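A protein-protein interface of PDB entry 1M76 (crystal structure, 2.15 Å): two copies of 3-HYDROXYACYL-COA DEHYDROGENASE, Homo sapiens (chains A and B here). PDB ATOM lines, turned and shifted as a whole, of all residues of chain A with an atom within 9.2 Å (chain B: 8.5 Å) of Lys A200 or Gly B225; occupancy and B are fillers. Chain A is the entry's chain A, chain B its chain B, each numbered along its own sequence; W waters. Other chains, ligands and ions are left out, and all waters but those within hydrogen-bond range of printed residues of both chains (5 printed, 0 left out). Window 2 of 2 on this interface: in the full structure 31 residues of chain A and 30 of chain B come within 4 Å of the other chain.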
ATOM      1  N   LEU A 139     -20.168 -15.753   5.991  1.00  0.00           N
ATOM      2  CA  LEU A 139     -20.122 -14.537   5.194  1.00  0.00           C
ATOM      3  C   LEU A 139     -20.690 -14.745   3.797  1.00  0.00           C
ATOM      4  O   LEU A 139     -20.856 -15.881   3.354  1.00  0.00           O
ATOM      5  CB  LEU A 139     -18.679 -14.030   5.122  1.00  0.00           C
ATOM      6  CG  LEU A 139     -18.028 -13.847   6.497  1.00  0.00           C
ATOM      7  CD1 LEU A 139     -16.618 -13.297   6.325  1.00  0.00           C
ATOM      8  CD2 LEU A 139     -18.878 -12.897   7.355  1.00  0.00           C
ATOM      9  N   GLN A 140     -21.010 -13.651   3.109  1.00  0.00           N
ATOM     10  CA  GLN A 140     -21.548 -13.769   1.763  1.00  0.00           C
ATOM     11  C   GLN A 140     -20.463 -13.722   0.690  1.00  0.00           C
ATOM     12  O   GLN A 140     -19.734 -12.738   0.560  1.00  0.00           O
ATOM     13  CB  GLN A 140     -22.577 -12.678   1.464  1.00  0.00           C
ATOM     14  CG  GLN A 140     -23.044 -12.786   0.026  1.00  0.00           C
ATOM     15  CD  GLN A 140     -24.229 -11.929  -0.307  1.00  0.00           C
ATOM     16  OE1 GLN A 140     -24.193 -10.711  -0.159  1.00  0.00           O
ATOM     17  NE2 GLN A 140     -25.292 -12.562  -0.779  1.00  0.00           N
ATOM     18  N   ILE A 141     -20.390 -14.798  -0.086  1.00  0.00           N
ATOM     19  CA  ILE A 141     -19.417 -14.944  -1.164  1.00  0.00           C
ATOM     20  C   ILE A 141     -19.431 -13.773  -2.150  1.00  0.00           C
ATOM     21  O   ILE A 141     -18.374 -13.254  -2.522  1.00  0.00           O
ATOM     22  CB  ILE A 141     -19.683 -16.247  -1.948  1.00  0.00           C
ATOM     23  CG1 ILE A 141     -19.834 -17.421  -0.973  1.00  0.00           C
ATOM     24  CG2 ILE A 141     -18.555 -16.503  -2.931  1.00  0.00           C
ATOM     25  CD1 ILE A 141     -18.582 -17.728  -0.163  1.00  0.00           C
ATOM     26  N   THR A 142     -20.626 -13.367  -2.577  1.00  0.00           N
ATOM     27  CA  THR A 142     -20.768 -12.265  -3.525  1.00  0.00           C
ATOM     28  C   THR A 142     -20.050 -11.023  -3.010  1.00  0.00           C
ATOM     29  O   THR A 142     -19.452 -10.267  -3.777  1.00  0.00           O
ATOM     30  CB  THR A 142     -22.247 -11.898  -3.747  1.00  0.00           C
ATOM     31  OG1 THR A 142     -22.969 -13.043  -4.218  1.00  0.00           O
ATOM     32  CG2 THR A 142     -22.362 -10.778  -4.769  1.00  0.00           C
ATOM     33  N   GLY A 156     -17.427 -19.948  -3.395  1.00  0.00           N
ATOM     34  CA  GLY A 156     -17.178 -20.466  -2.067  1.00  0.00           C
ATOM     35  C   GLY A 156     -16.925 -21.961  -2.148  1.00  0.00           C
ATOM     36  O   GLY A 156     -17.548 -22.654  -2.953  1.00  0.00           O
ATOM     37  N   GLU A 170     -19.440 -27.810   0.442  1.00  0.00           N
ATOM     38  CA  GLU A 170     -20.490 -26.993  -0.158  1.00  0.00           C
ATOM     39  C   GLU A 170     -19.852 -26.065  -1.188  1.00  0.00           C
ATOM     40  O   GLU A 170     -18.940 -25.309  -0.868  1.00  0.00           O
ATOM     41  CB  GLU A 170     -21.207 -26.157   0.909  1.00  0.00           C
ATOM     42  CG  GLU A 170     -21.924 -26.970   1.974  1.00  0.00           C
ATOM     43  CD  GLU A 170     -22.521 -26.093   3.064  1.00  0.00           C
ATOM     44  OE1 GLU A 170     -21.777 -25.268   3.635  1.00  0.00           O
ATOM     45  OE2 GLU A 170     -23.727 -26.227   3.354  1.00  0.00           O
ATOM     46  N   VAL A 171     -20.329 -26.131  -2.426  1.00  0.00           N
ATOM     47  CA  VAL A 171     -19.804 -25.288  -3.493  1.00  0.00           C
ATOM     48  C   VAL A 171     -20.791 -24.154  -3.725  1.00  0.00           C
ATOM     49  O   VAL A 171     -21.942 -24.387  -4.092  1.00  0.00           O
ATOM     50  CB  VAL A 171     -19.629 -26.088  -4.790  1.00  0.00           C
ATOM     51  CG1 VAL A 171     -19.001 -25.217  -5.855  1.00  0.00           C
ATOM     52  CG2 VAL A 171     -18.781 -27.311  -4.519  1.00  0.00           C
ATOM     53  N   ILE A 172     -20.335 -22.922  -3.518  1.00  0.00           N
ATOM     54  CA  ILE A 172     -21.213 -21.772  -3.664  1.00  0.00           C
ATOM     55  C   ILE A 172     -20.891 -20.829  -4.815  1.00  0.00           C
ATOM     56  O   ILE A 172     -19.835 -20.189  -4.849  1.00  0.00           O
ATOM     57  CB  ILE A 172     -21.243 -20.934  -2.363  1.00  0.00           C
ATOM     58  CG1 ILE A 172     -21.524 -21.838  -1.161  1.00  0.00           C
ATOM     59  CG2 ILE A 172     -22.302 -19.856  -2.463  1.00  0.00           C
ATOM     60  CD1 ILE A 172     -20.294 -22.521  -0.612  1.00  0.00           C
ATOM     61  N   LYS A 173     -21.830 -20.741  -5.747  1.00  0.00           N
ATOM     62  CA  LYS A 173     -21.712 -19.862  -6.901  1.00  0.00           C
ATOM     63  C   LYS A 173     -22.314 -18.514  -6.545  1.00  0.00           C
ATOM     64  O   LYS A 173     -23.255 -18.443  -5.756  1.00  0.00           O
ATOM     65  CB  LYS A 173     -22.539 -20.387  -8.072  1.00  0.00           C
ATOM     66  CG  LYS A 173     -21.934 -21.427  -8.966  1.00  0.00           C
ATOM     67  CD  LYS A 173     -23.045 -21.918  -9.891  1.00  0.00           C
ATOM     68  CE  LYS A 173     -22.511 -22.516 -11.170  1.00  0.00           C
ATOM     69  NZ  LYS A 173     -23.621 -23.043 -12.019  1.00  0.00           N
ATOM     70  N   THR A 174     -21.773 -17.448  -7.122  1.00  0.00           N
ATOM     71  CA  THR A 174     -22.363 -16.129  -6.935  1.00  0.00           C
ATOM     72  C   THR A 174     -22.987 -15.979  -8.320  1.00  0.00           C
ATOM     73  O   THR A 174     -22.696 -16.774  -9.215  1.00  0.00           O
ATOM     74  CB  THR A 174     -21.319 -15.008  -6.757  1.00  0.00           C
ATOM     75  OG1 THR A 174     -20.712 -14.717  -8.023  1.00  0.00           O
ATOM     76  CG2 THR A 174     -20.256 -15.416  -5.755  1.00  0.00           C
ATOM     77  N   PRO A 175     -23.854 -14.983  -8.521  1.00  0.00           N
ATOM     78  CA  PRO A 175     -24.429 -14.866  -9.863  1.00  0.00           C
ATOM     79  C   PRO A 175     -23.367 -14.542 -10.913  1.00  0.00           C
ATOM     80  O   PRO A 175     -23.621 -14.641 -12.111  1.00  0.00           O
ATOM     81  CB  PRO A 175     -25.455 -13.750  -9.697  1.00  0.00           C
ATOM     82  CG  PRO A 175     -25.895 -13.922  -8.264  1.00  0.00           C
ATOM     83  CD  PRO A 175     -24.572 -14.130  -7.559  1.00  0.00           C
ATOM     84  N   PHE A 182     -17.155 -22.989 -11.681  1.00  0.00           N
ATOM     85  CA  PHE A 182     -17.980 -23.893 -10.882  1.00  0.00           C
ATOM     86  C   PHE A 182     -17.545 -25.336 -11.112  1.00  0.00           C
ATOM     87  O   PHE A 182     -17.231 -26.060 -10.168  1.00  0.00           O
ATOM     88  CB  PHE A 182     -19.458 -23.747 -11.263  1.00  0.00           C
ATOM     89  CG  PHE A 182     -20.369 -24.732 -10.574  1.00  0.00           C
ATOM     90  CD1 PHE A 182     -20.592 -24.657  -9.202  1.00  0.00           C
ATOM     91  CD2 PHE A 182     -21.012 -25.729 -11.302  1.00  0.00           C
ATOM     92  CE1 PHE A 182     -21.448 -25.561  -8.559  1.00  0.00           C
ATOM     93  CE2 PHE A 182     -21.871 -26.642 -10.674  1.00  0.00           C
ATOM     94  CZ  PHE A 182     -22.090 -26.557  -9.297  1.00  0.00           C
ATOM     95  N   VAL A 197     -21.805 -30.382  -2.948  1.00  0.00           N
ATOM     96  CA  VAL A 197     -23.220 -30.033  -3.038  1.00  0.00           C
ATOM     97  C   VAL A 197     -23.284 -28.549  -3.373  1.00  0.00           C
ATOM     98  O   VAL A 197     -22.804 -27.713  -2.602  1.00  0.00           O
ATOM     99  CB  VAL A 197     -23.965 -30.254  -1.701  1.00  0.00           C
ATOM    100  CG1 VAL A 197     -25.391 -29.744  -1.816  1.00  0.00           C
ATOM    101  CG2 VAL A 197     -23.958 -31.727  -1.327  1.00  0.00           C
ATOM    102  N   SER A 198     -23.865 -28.224  -4.521  1.00  0.00           N
ATOM    103  CA  SER A 198     -23.984 -26.832  -4.945  1.00  0.00           C
ATOM    104  C   SER A 198     -25.013 -26.089  -4.085  1.00  0.00           C
ATOM    105  O   SER A 198     -26.159 -26.522  -3.968  1.00  0.00           O
ATOM    106  CB  SER A 198     -24.399 -26.775  -6.416  1.00  0.00           C
ATOM    107  OG  SER A 198     -24.474 -25.441  -6.874  1.00  0.00           O
ATOM    108  N   CYS A 199     -24.600 -24.973  -3.490  1.00  0.00           N
ATOM    109  CA  CYS A 199     -25.492 -24.184  -2.640  1.00  0.00           C
ATOM    110  C   CYS A 199     -25.604 -22.741  -3.109  1.00  0.00           C
ATOM    111  O   CYS A 199     -24.698 -22.216  -3.766  1.00  0.00           O
ATOM    112  CB  CYS A 199     -24.989 -24.176  -1.196  1.00  0.00           C
ATOM    113  SG  CYS A 199     -24.832 -25.795  -0.420  1.00  0.00           S
ATOM    114  N   LYS A 200     -26.719 -22.100  -2.774  1.00  0.00           N
ATOM    115  CA  LYS A 200     -26.910 -20.701  -3.131  1.00  0.00           C
ATOM    116  C   LYS A 200     -26.100 -19.888  -2.128  1.00  0.00           C
ATOM    117  O   LYS A 200     -25.747 -20.383  -1.057  1.00  0.00           O
ATOM    118  CB  LYS A 200     -28.381 -20.299  -3.029  1.00  0.00           C
ATOM    119  CG  LYS A 200     -29.314 -21.071  -3.936  1.00  0.00           C
ATOM    120  CD  LYS A 200     -30.710 -20.472  -3.912  1.00  0.00           C
ATOM    121  CE  LYS A 200     -31.678 -21.281  -4.765  1.00  0.00           C
ATOM    122  NZ  LYS A 200     -32.981 -20.567  -4.889  1.00  0.00           N
ATOM    123  N   ASP A 201     -25.805 -18.641  -2.474  1.00  0.00           N
ATOM    124  CA  ASP A 201     -25.034 -17.781  -1.588  1.00  0.00           C
ATOM    125  C   ASP A 201     -25.947 -17.128  -0.549  1.00  0.00           C
ATOM    126  O   ASP A 201     -26.258 -15.938  -0.635  1.00  0.00           O
ATOM    127  CB  ASP A 201     -24.301 -16.717  -2.410  1.00  0.00           C
ATOM    128  CG  ASP A 201     -23.341 -15.883  -1.574  1.00  0.00           C
ATOM    129  OD1 ASP A 201     -22.944 -16.339  -0.477  1.00  0.00           O
ATOM    130  OD2 ASP A 201     -22.970 -14.779  -2.031  1.00  0.00           O
ATOM    131  N   THR A 202     -26.389 -17.927   0.419  1.00  0.00           N
ATOM    132  CA  THR A 202     -27.248 -17.447   1.500  1.00  0.00           C
ATOM    133  C   THR A 202     -26.496 -17.672   2.805  1.00  0.00           C
ATOM    134  O   THR A 202     -25.758 -18.642   2.937  1.00  0.00           O
ATOM    135  CB  THR A 202     -28.595 -18.205   1.544  1.00  0.00           C
ATOM    136  OG1 THR A 202     -28.358 -19.617   1.620  1.00  0.00           O
ATOM    137  CG2 THR A 202     -29.416 -17.892   0.305  1.00  0.00           C
ATOM    138  N   PRO A 203     -26.683 -16.784   3.791  1.00  0.00           N
ATOM    139  CA  PRO A 203     -26.001 -16.900   5.084  1.00  0.00           C
ATOM    140  C   PRO A 203     -25.955 -18.283   5.738  1.00  0.00           C
ATOM    141  O   PRO A 203     -26.984 -18.846   6.125  1.00  0.00           O
ATOM    142  CB  PRO A 203     -26.707 -15.848   5.955  1.00  0.00           C
ATOM    143  CG  PRO A 203     -28.025 -15.617   5.261  1.00  0.00           C
ATOM    144  CD  PRO A 203     -27.672 -15.691   3.809  1.00  0.00           C
ATOM    145  N   GLY A 204     -24.745 -18.819   5.862  1.00  0.00           N
ATOM    146  CA  GLY A 204     -24.570 -20.124   6.479  1.00  0.00           C
ATOM    147  C   GLY A 204     -24.829 -21.267   5.516  1.00  0.00           C
ATOM    148  O   GLY A 204     -24.729 -22.442   5.886  1.00  0.00           O
ATOM    149  N   PHE A 205     -25.161 -20.918   4.277  1.00  0.00           N
ATOM    150  CA  PHE A 205     -25.438 -21.909   3.248  1.00  0.00           C
ATOM    151  C   PHE A 205     -26.428 -22.926   3.811  1.00  0.00           C
ATOM    152  O   PHE A 205     -27.516 -22.540   4.251  1.00  0.00           O
ATOM    153  CB  PHE A 205     -24.122 -22.559   2.811  1.00  0.00           C
ATOM    154  CG  PHE A 205     -23.014 -21.552   2.576  1.00  0.00           C
ATOM    155  CD1 PHE A 205     -23.181 -20.518   1.650  1.00  0.00           C
ATOM    156  CD2 PHE A 205     -21.835 -21.603   3.311  1.00  0.00           C
ATOM    157  CE1 PHE A 205     -22.185 -19.545   1.470  1.00  0.00           C
ATOM    158  CE2 PHE A 205     -20.833 -20.639   3.140  1.00  0.00           C
ATOM    159  CZ  PHE A 205     -21.009 -19.609   2.219  1.00  0.00           C
ATOM    160  N   ILE A 206     -26.073 -24.206   3.819  1.00  0.00           N
ATOM    161  CA  ILE A 206     -27.001 -25.188   4.354  1.00  0.00           C
ATOM    162  C   ILE A 206     -26.694 -25.598   5.777  1.00  0.00           C
ATOM    163  O   ILE A 206     -27.439 -25.276   6.695  1.00  0.00           O
ATOM    164  CB  ILE A 206     -27.057 -26.490   3.517  1.00  0.00           C
ATOM    165  CG1 ILE A 206     -27.723 -26.243   2.161  1.00  0.00           C
ATOM    166  CG2 ILE A 206     -27.864 -27.545   4.273  1.00  0.00           C
ATOM    167  CD1 ILE A 206     -27.754 -27.492   1.281  1.00  0.00           C
ATOM    168  N   VAL A 207     -25.590 -26.310   5.949  1.00  0.00           N
ATOM    169  CA  VAL A 207     -25.214 -26.827   7.251  1.00  0.00           C
ATOM    170  C   VAL A 207     -25.161 -25.814   8.390  1.00  0.00           C
ATOM    171  O   VAL A 207     -25.880 -25.966   9.374  1.00  0.00           O
ATOM    172  CB  VAL A 207     -23.877 -27.586   7.158  1.00  0.00           C
ATOM    173  CG1 VAL A 207     -23.520 -28.181   8.514  1.00  0.00           C
ATOM    174  CG2 VAL A 207     -23.990 -28.688   6.108  1.00  0.00           C
ATOM    175  N   ARG A 209     -26.259 -22.701   8.592  1.00  0.00           N
ATOM    176  CA  ARG A 209     -27.527 -22.014   8.783  1.00  0.00           C
ATOM    177  C   ARG A 209     -28.438 -22.817   9.723  1.00  0.00           C
ATOM    178  O   ARG A 209     -29.289 -22.249  10.411  1.00  0.00           O
ATOM    179  CB  ARG A 209     -28.218 -21.821   7.435  1.00  0.00           C
ATOM    180  CG  ARG A 209     -29.574 -21.150   7.515  1.00  0.00           C
ATOM    181  CD  ARG A 209     -29.470 -19.722   7.995  1.00  0.00           C
ATOM    182  NE  ARG A 209     -30.788 -19.103   8.107  1.00  0.00           N
ATOM    183  CZ  ARG A 209     -31.692 -19.419   9.030  1.00  0.00           C
ATOM    184  NH1 ARG A 209     -31.420 -20.351   9.936  1.00  0.00           N
ATOM    185  NH2 ARG A 209     -32.876 -18.813   9.034  1.00  0.00           N
ATOM    186  N   ALA B 218     -35.059 -26.401   9.188  1.00  0.00           N
ATOM    187  CA  ALA B 218     -34.735 -27.153   7.982  1.00  0.00           C
ATOM    188  C   ALA B 218     -35.902 -26.972   7.018  1.00  0.00           C
ATOM    189  O   ALA B 218     -35.705 -26.677   5.843  1.00  0.00           O
ATOM    190  CB  ALA B 218     -34.545 -28.628   8.308  1.00  0.00           C
ATOM    191  N   ILE B 219     -37.124 -27.127   7.524  1.00  0.00           N
ATOM    192  CA  ILE B 219     -38.299 -26.961   6.673  1.00  0.00           C
ATOM    193  C   ILE B 219     -38.376 -25.539   6.106  1.00  0.00           C
ATOM    194  O   ILE B 219     -38.607 -25.355   4.912  1.00  0.00           O
ATOM    195  CB  ILE B 219     -39.617 -27.245   7.433  1.00  0.00           C
ATOM    196  CG1 ILE B 219     -39.630 -28.682   7.959  1.00  0.00           C
ATOM    197  CG2 ILE B 219     -40.802 -27.053   6.494  1.00  0.00           C
ATOM    198  CD1 ILE B 219     -40.859 -29.011   8.798  1.00  0.00           C
ATOM    199  N   ARG B 220     -38.189 -24.536   6.960  1.00  0.00           N
ATOM    200  CA  ARG B 220     -38.258 -23.153   6.506  1.00  0.00           C
ATOM    201  C   ARG B 220     -37.219 -22.841   5.427  1.00  0.00           C
ATOM    202  O   ARG B 220     -37.503 -22.107   4.483  1.00  0.00           O
ATOM    203  CB  ARG B 220     -38.099 -22.195   7.688  1.00  0.00           C
ATOM    204  CG  ARG B 220     -39.182 -22.362   8.741  1.00  0.00           C
ATOM    205  CD  ARG B 220     -39.177 -21.237   9.764  1.00  0.00           C
ATOM    206  NE  ARG B 220     -40.066 -21.540  10.883  1.00  0.00           N
ATOM    207  CZ  ARG B 220     -39.659 -21.987  12.067  1.00  0.00           C
ATOM    208  NH1 ARG B 220     -38.370 -22.179  12.299  1.00  0.00           N
ATOM    209  NH2 ARG B 220     -40.548 -22.257  13.017  1.00  0.00           N
ATOM    210  N   LEU B 221     -36.022 -23.394   5.570  1.00  0.00           N
ATOM    211  CA  LEU B 221     -34.971 -23.174   4.582  1.00  0.00           C
ATOM    212  C   LEU B 221     -35.449 -23.728   3.232  1.00  0.00           C
ATOM    213  O   LEU B 221     -35.257 -23.104   2.185  1.00  0.00           O
ATOM    214  CB  LEU B 221     -33.685 -23.874   5.023  1.00  0.00           C
ATOM    215  CG  LEU B 221     -32.411 -23.677   4.192  1.00  0.00           C
ATOM    216  CD1 LEU B 221     -31.209 -24.084   5.022  1.00  0.00           C
ATOM    217  CD2 LEU B 221     -32.471 -24.495   2.924  1.00  0.00           C
ATOM    218  N   TYR B 222     -36.080 -24.897   3.273  1.00  0.00           N
ATOM    219  CA  TYR B 222     -36.602 -25.546   2.074  1.00  0.00           C
ATOM    220  C   TYR B 222     -37.743 -24.744   1.450  1.00  0.00           C
ATOM    221  O   TYR B 222     -37.772 -24.535   0.233  1.00  0.00           O
ATOM    222  CB  TYR B 222     -37.094 -26.949   2.421  1.00  0.00           C
ATOM    223  CG  TYR B 222     -38.014 -27.568   1.389  1.00  0.00           C
ATOM    224  CD1 TYR B 222     -37.582 -27.786   0.080  1.00  0.00           C
ATOM    225  CD2 TYR B 222     -39.308 -27.958   1.730  1.00  0.00           C
ATOM    226  CE1 TYR B 222     -38.415 -28.383  -0.864  1.00  0.00           C
ATOM    227  CE2 TYR B 222     -40.153 -28.556   0.792  1.00  0.00           C
ATOM    228  CZ  TYR B 222     -39.697 -28.766  -0.502  1.00  0.00           C
ATOM    229  OH  TYR B 222     -40.512 -29.368  -1.432  1.00  0.00           O
ATOM    230  N   GLU B 223     -38.681 -24.294   2.285  1.00  0.00           N
ATOM    231  CA  GLU B 223     -39.824 -23.518   1.808  1.00  0.00           C
ATOM    232  C   GLU B 223     -39.372 -22.195   1.217  1.00  0.00           C
ATOM    233  O   GLU B 223     -40.041 -21.619   0.371  1.00  0.00           O
ATOM    234  CB  GLU B 223     -40.815 -23.264   2.952  1.00  0.00           C
ATOM    235  CG  GLU B 223     -41.483 -24.532   3.473  1.00  0.00           C
ATOM    236  CD  GLU B 223     -42.458 -24.264   4.603  1.00  0.00           C
ATOM    237  OE1 GLU B 223     -42.027 -23.778   5.672  1.00  0.00           O
ATOM    238  OE2 GLU B 223     -43.658 -24.537   4.424  1.00  0.00           O
ATOM    239  N   ARG B 224     -38.226 -21.717   1.674  1.00  0.00           N
ATOM    240  CA  ARG B 224     -37.662 -20.465   1.186  1.00  0.00           C
ATOM    241  C   ARG B 224     -37.195 -20.708  -0.253  1.00  0.00           C
ATOM    242  O   ARG B 224     -37.068 -19.779  -1.049  1.00  0.00           O
ATOM    243  CB  ARG B 224     -36.474 -20.080   2.074  1.00  0.00           C
ATOM    244  CG  ARG B 224     -36.242 -18.600   2.263  1.00  0.00           C
ATOM    245  CD  ARG B 224     -35.854 -18.310   3.714  1.00  0.00           C
ATOM    246  NE  ARG B 224     -34.718 -19.113   4.180  1.00  0.00           N
ATOM    247  CZ  ARG B 224     -34.629 -19.627   5.405  1.00  0.00           C
ATOM    248  NH1 ARG B 224     -35.604 -19.428   6.279  1.00  0.00           N
ATOM    249  NH2 ARG B 224     -33.566 -20.337   5.764  1.00  0.00           N
ATOM    250  N   GLY B 225     -36.963 -21.974  -0.584  1.00  0.00           N
ATOM    251  CA  GLY B 225     -36.488 -22.318  -1.915  1.00  0.00           C
ATOM    252  C   GLY B 225     -34.968 -22.245  -1.976  1.00  0.00           C
ATOM    253  O   GLY B 225     -34.371 -22.344  -3.052  1.00  0.00           O
ATOM    254  N   ASP B 226     -34.338 -22.071  -0.816  1.00  0.00           N
ATOM    255  CA  ASP B 226     -32.883 -21.980  -0.749  1.00  0.00           C
ATOM    256  C   ASP B 226     -32.182 -23.282  -1.132  1.00  0.00           C
ATOM    257  O   ASP B 226     -31.065 -23.258  -1.658  1.00  0.00           O
ATOM    258  CB  ASP B 226     -32.437 -21.540   0.652  1.00  0.00           C
ATOM    259  CG  ASP B 226     -32.830 -20.112   0.964  1.00  0.00           C
ATOM    260  OD1 ASP B 226     -33.133 -19.367   0.010  1.00  0.00           O
ATOM    261  OD2 ASP B 226     -32.824 -19.727   2.150  1.00  0.00           O
ATOM    262  N   ALA B 227     -32.833 -24.413  -0.866  1.00  0.00           N
ATOM    263  CA  ALA B 227     -32.269 -25.721  -1.195  1.00  0.00           C
ATOM    264  C   ALA B 227     -33.340 -26.810  -1.188  1.00  0.00           C
ATOM    265  O   ALA B 227     -34.422 -26.629  -0.629  1.00  0.00           O
ATOM    266  CB  ALA B 227     -31.164 -26.081  -0.211  1.00  0.00           C
ATOM    267  N   SER B 228     -33.023 -27.941  -1.804  1.00  0.00           N
ATOM    268  CA  SER B 228     -33.943 -29.070  -1.870  1.00  0.00           C
ATOM    269  C   SER B 228     -33.844 -29.905  -0.600  1.00  0.00           C
ATOM    270  O   SER B 228     -32.819 -29.892   0.091  1.00  0.00           O
ATOM    271  CB  SER B 228     -33.607 -29.963  -3.065  1.00  0.00           C
ATOM    272  OG  SER B 228     -32.360 -30.609  -2.865  1.00  0.00           O
ATOM    273  N   ASP B 231     -30.854 -32.315  -0.885  1.00  0.00           N
ATOM    274  CA  ASP B 231     -29.534 -31.748  -0.615  1.00  0.00           C
ATOM    275  C   ASP B 231     -29.393 -31.386   0.864  1.00  0.00           C
ATOM    276  O   ASP B 231     -28.338 -31.600   1.462  1.00  0.00           O
ATOM    277  CB  ASP B 231     -29.280 -30.523  -1.499  1.00  0.00           C
ATOM    278  CG  ASP B 231     -29.069 -30.896  -2.961  1.00  0.00           C
ATOM    279  OD1 ASP B 231     -28.648 -32.041  -3.227  1.00  0.00           O
ATOM    280  OD2 ASP B 231     -29.310 -30.045  -3.841  1.00  0.00           O
ATOM    281  N   ILE B 232     -30.453 -30.844   1.461  1.00  0.00           N
ATOM    282  CA  ILE B 232     -30.398 -30.505   2.879  1.00  0.00           C
ATOM    283  C   ILE B 232     -30.114 -31.775   3.682  1.00  0.00           C
ATOM    284  O   ILE B 232     -29.290 -31.768   4.598  1.00  0.00           O
ATOM    285  CB  ILE B 232     -31.724 -29.869   3.371  1.00  0.00           C
ATOM    286  CG1 ILE B 232     -31.887 -28.476   2.751  1.00  0.00           C
ATOM    287  CG2 ILE B 232     -31.711 -29.745   4.889  1.00  0.00           C
ATOM    288  CD1 ILE B 232     -33.288 -27.894   2.857  1.00  0.00           C
HETATM  289  O   HOH W   1     -35.791 -19.084   9.173  1.00  0.00           O
HETATM  290  O   HOH W   2     -27.256 -28.794  -4.997  1.00  0.00           O
HETATM  291  O   HOH W   3     -28.434 -23.830  -1.129  1.00  0.00           O
HETATM  292  O   HOH W   4     -33.886 -19.197  -2.739  1.00  0.00           O
HETATM  293  O   HOH W   5     -34.095 -21.690   8.014  1.00  0.00           O
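Water W2 lies within hydrogen-bond range of OD2 of Asp B231 and O of Ser A198. Water W5 lies within hydrogen-bond range of NH2 of Arg B224 (2.7 Å) and NH2 of Arg A209 (3.3 Å). Water W4 lies within hydrogen-bond range of the side-chain amino group of Lys A200 (2.7 Å), the side-chain carboxylate of Asp B226 (2.9 Å) and the backbone carbonyl oxygen of Gly B225 (3.2 Å). Water W3 lies within hydrogen-bond range of O of Asp B226 (2.7 Å) and N of Lys A200 (2.9 Å). Water W1 lies within hydrogen-bond range of NH1 of Arg B224 (2.9 Å) and NH2 of Arg A209 (2.9 Å).
The side-chain carboxylate (OE2) of Glu A170 lies within hydrogen-bond range of the backbone NH (N) of Ile A206. N of Val A171 lies within hydrogen-bond range of O of Val A197, at 2.9 Å. SG of Cys A199 is in hydrogen-bond range of O of Val A197 (3.5 Å). The backbone carbonyl oxygen (O) of Gly A204 lies within hydrogen-bond range of the backbone NH (N) of Arg A209, 3.1 Å away. The backbone carbonyl oxygen (O) of Leu B221 lies within hydrogen-bond range of the backbone NH (N) of Asp B226 (3.3 Å). The guanidinium group (NE) of Arg B224 lies within salt-bridge range of the side-chain carboxylate (OD2) of Asp B226 (2.8 Å).
CG1 of Val A197 touches CB of Asp B231, 3.98 Å away. Lys A200 touches Asp B226 (CD to O, 3.6 Å). Ala B227 touches Ile A206 (CB to CD1, 3.98 Å). Arg B224 touches Arg A209 (NH2 to NH2, 3.7 Å).
Hydrophobic or aromatic side chains of chain A within 4 Å of the printed part of chain B: Val A197 and Ile A206. Among the printed residues, 5 pairs touch across the chains. Among the printed residues, no Asp or Glu carboxylate lies within 4 Å of a Lys or Arg side-chain nitrogen of the other chain.
Lys A200 touches two residues of chain B. Of the printed residues of chain B, Val A197 touches Asp B231. Of the printed residues of chain A, Arg B224 touches Arg A209 (3.7 Å). The nearest residue of chain A that does not touch Gly B225 is Thr A202 (7.4 Å). The nearest printed residue of chain A that does not touch Ala B227 is Lys A200 (5.1 Å).
O of Gly B225 is in hydrogen-bond range of NZ of Lys A200 (2.9 Å).
No position is printed for both chains.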
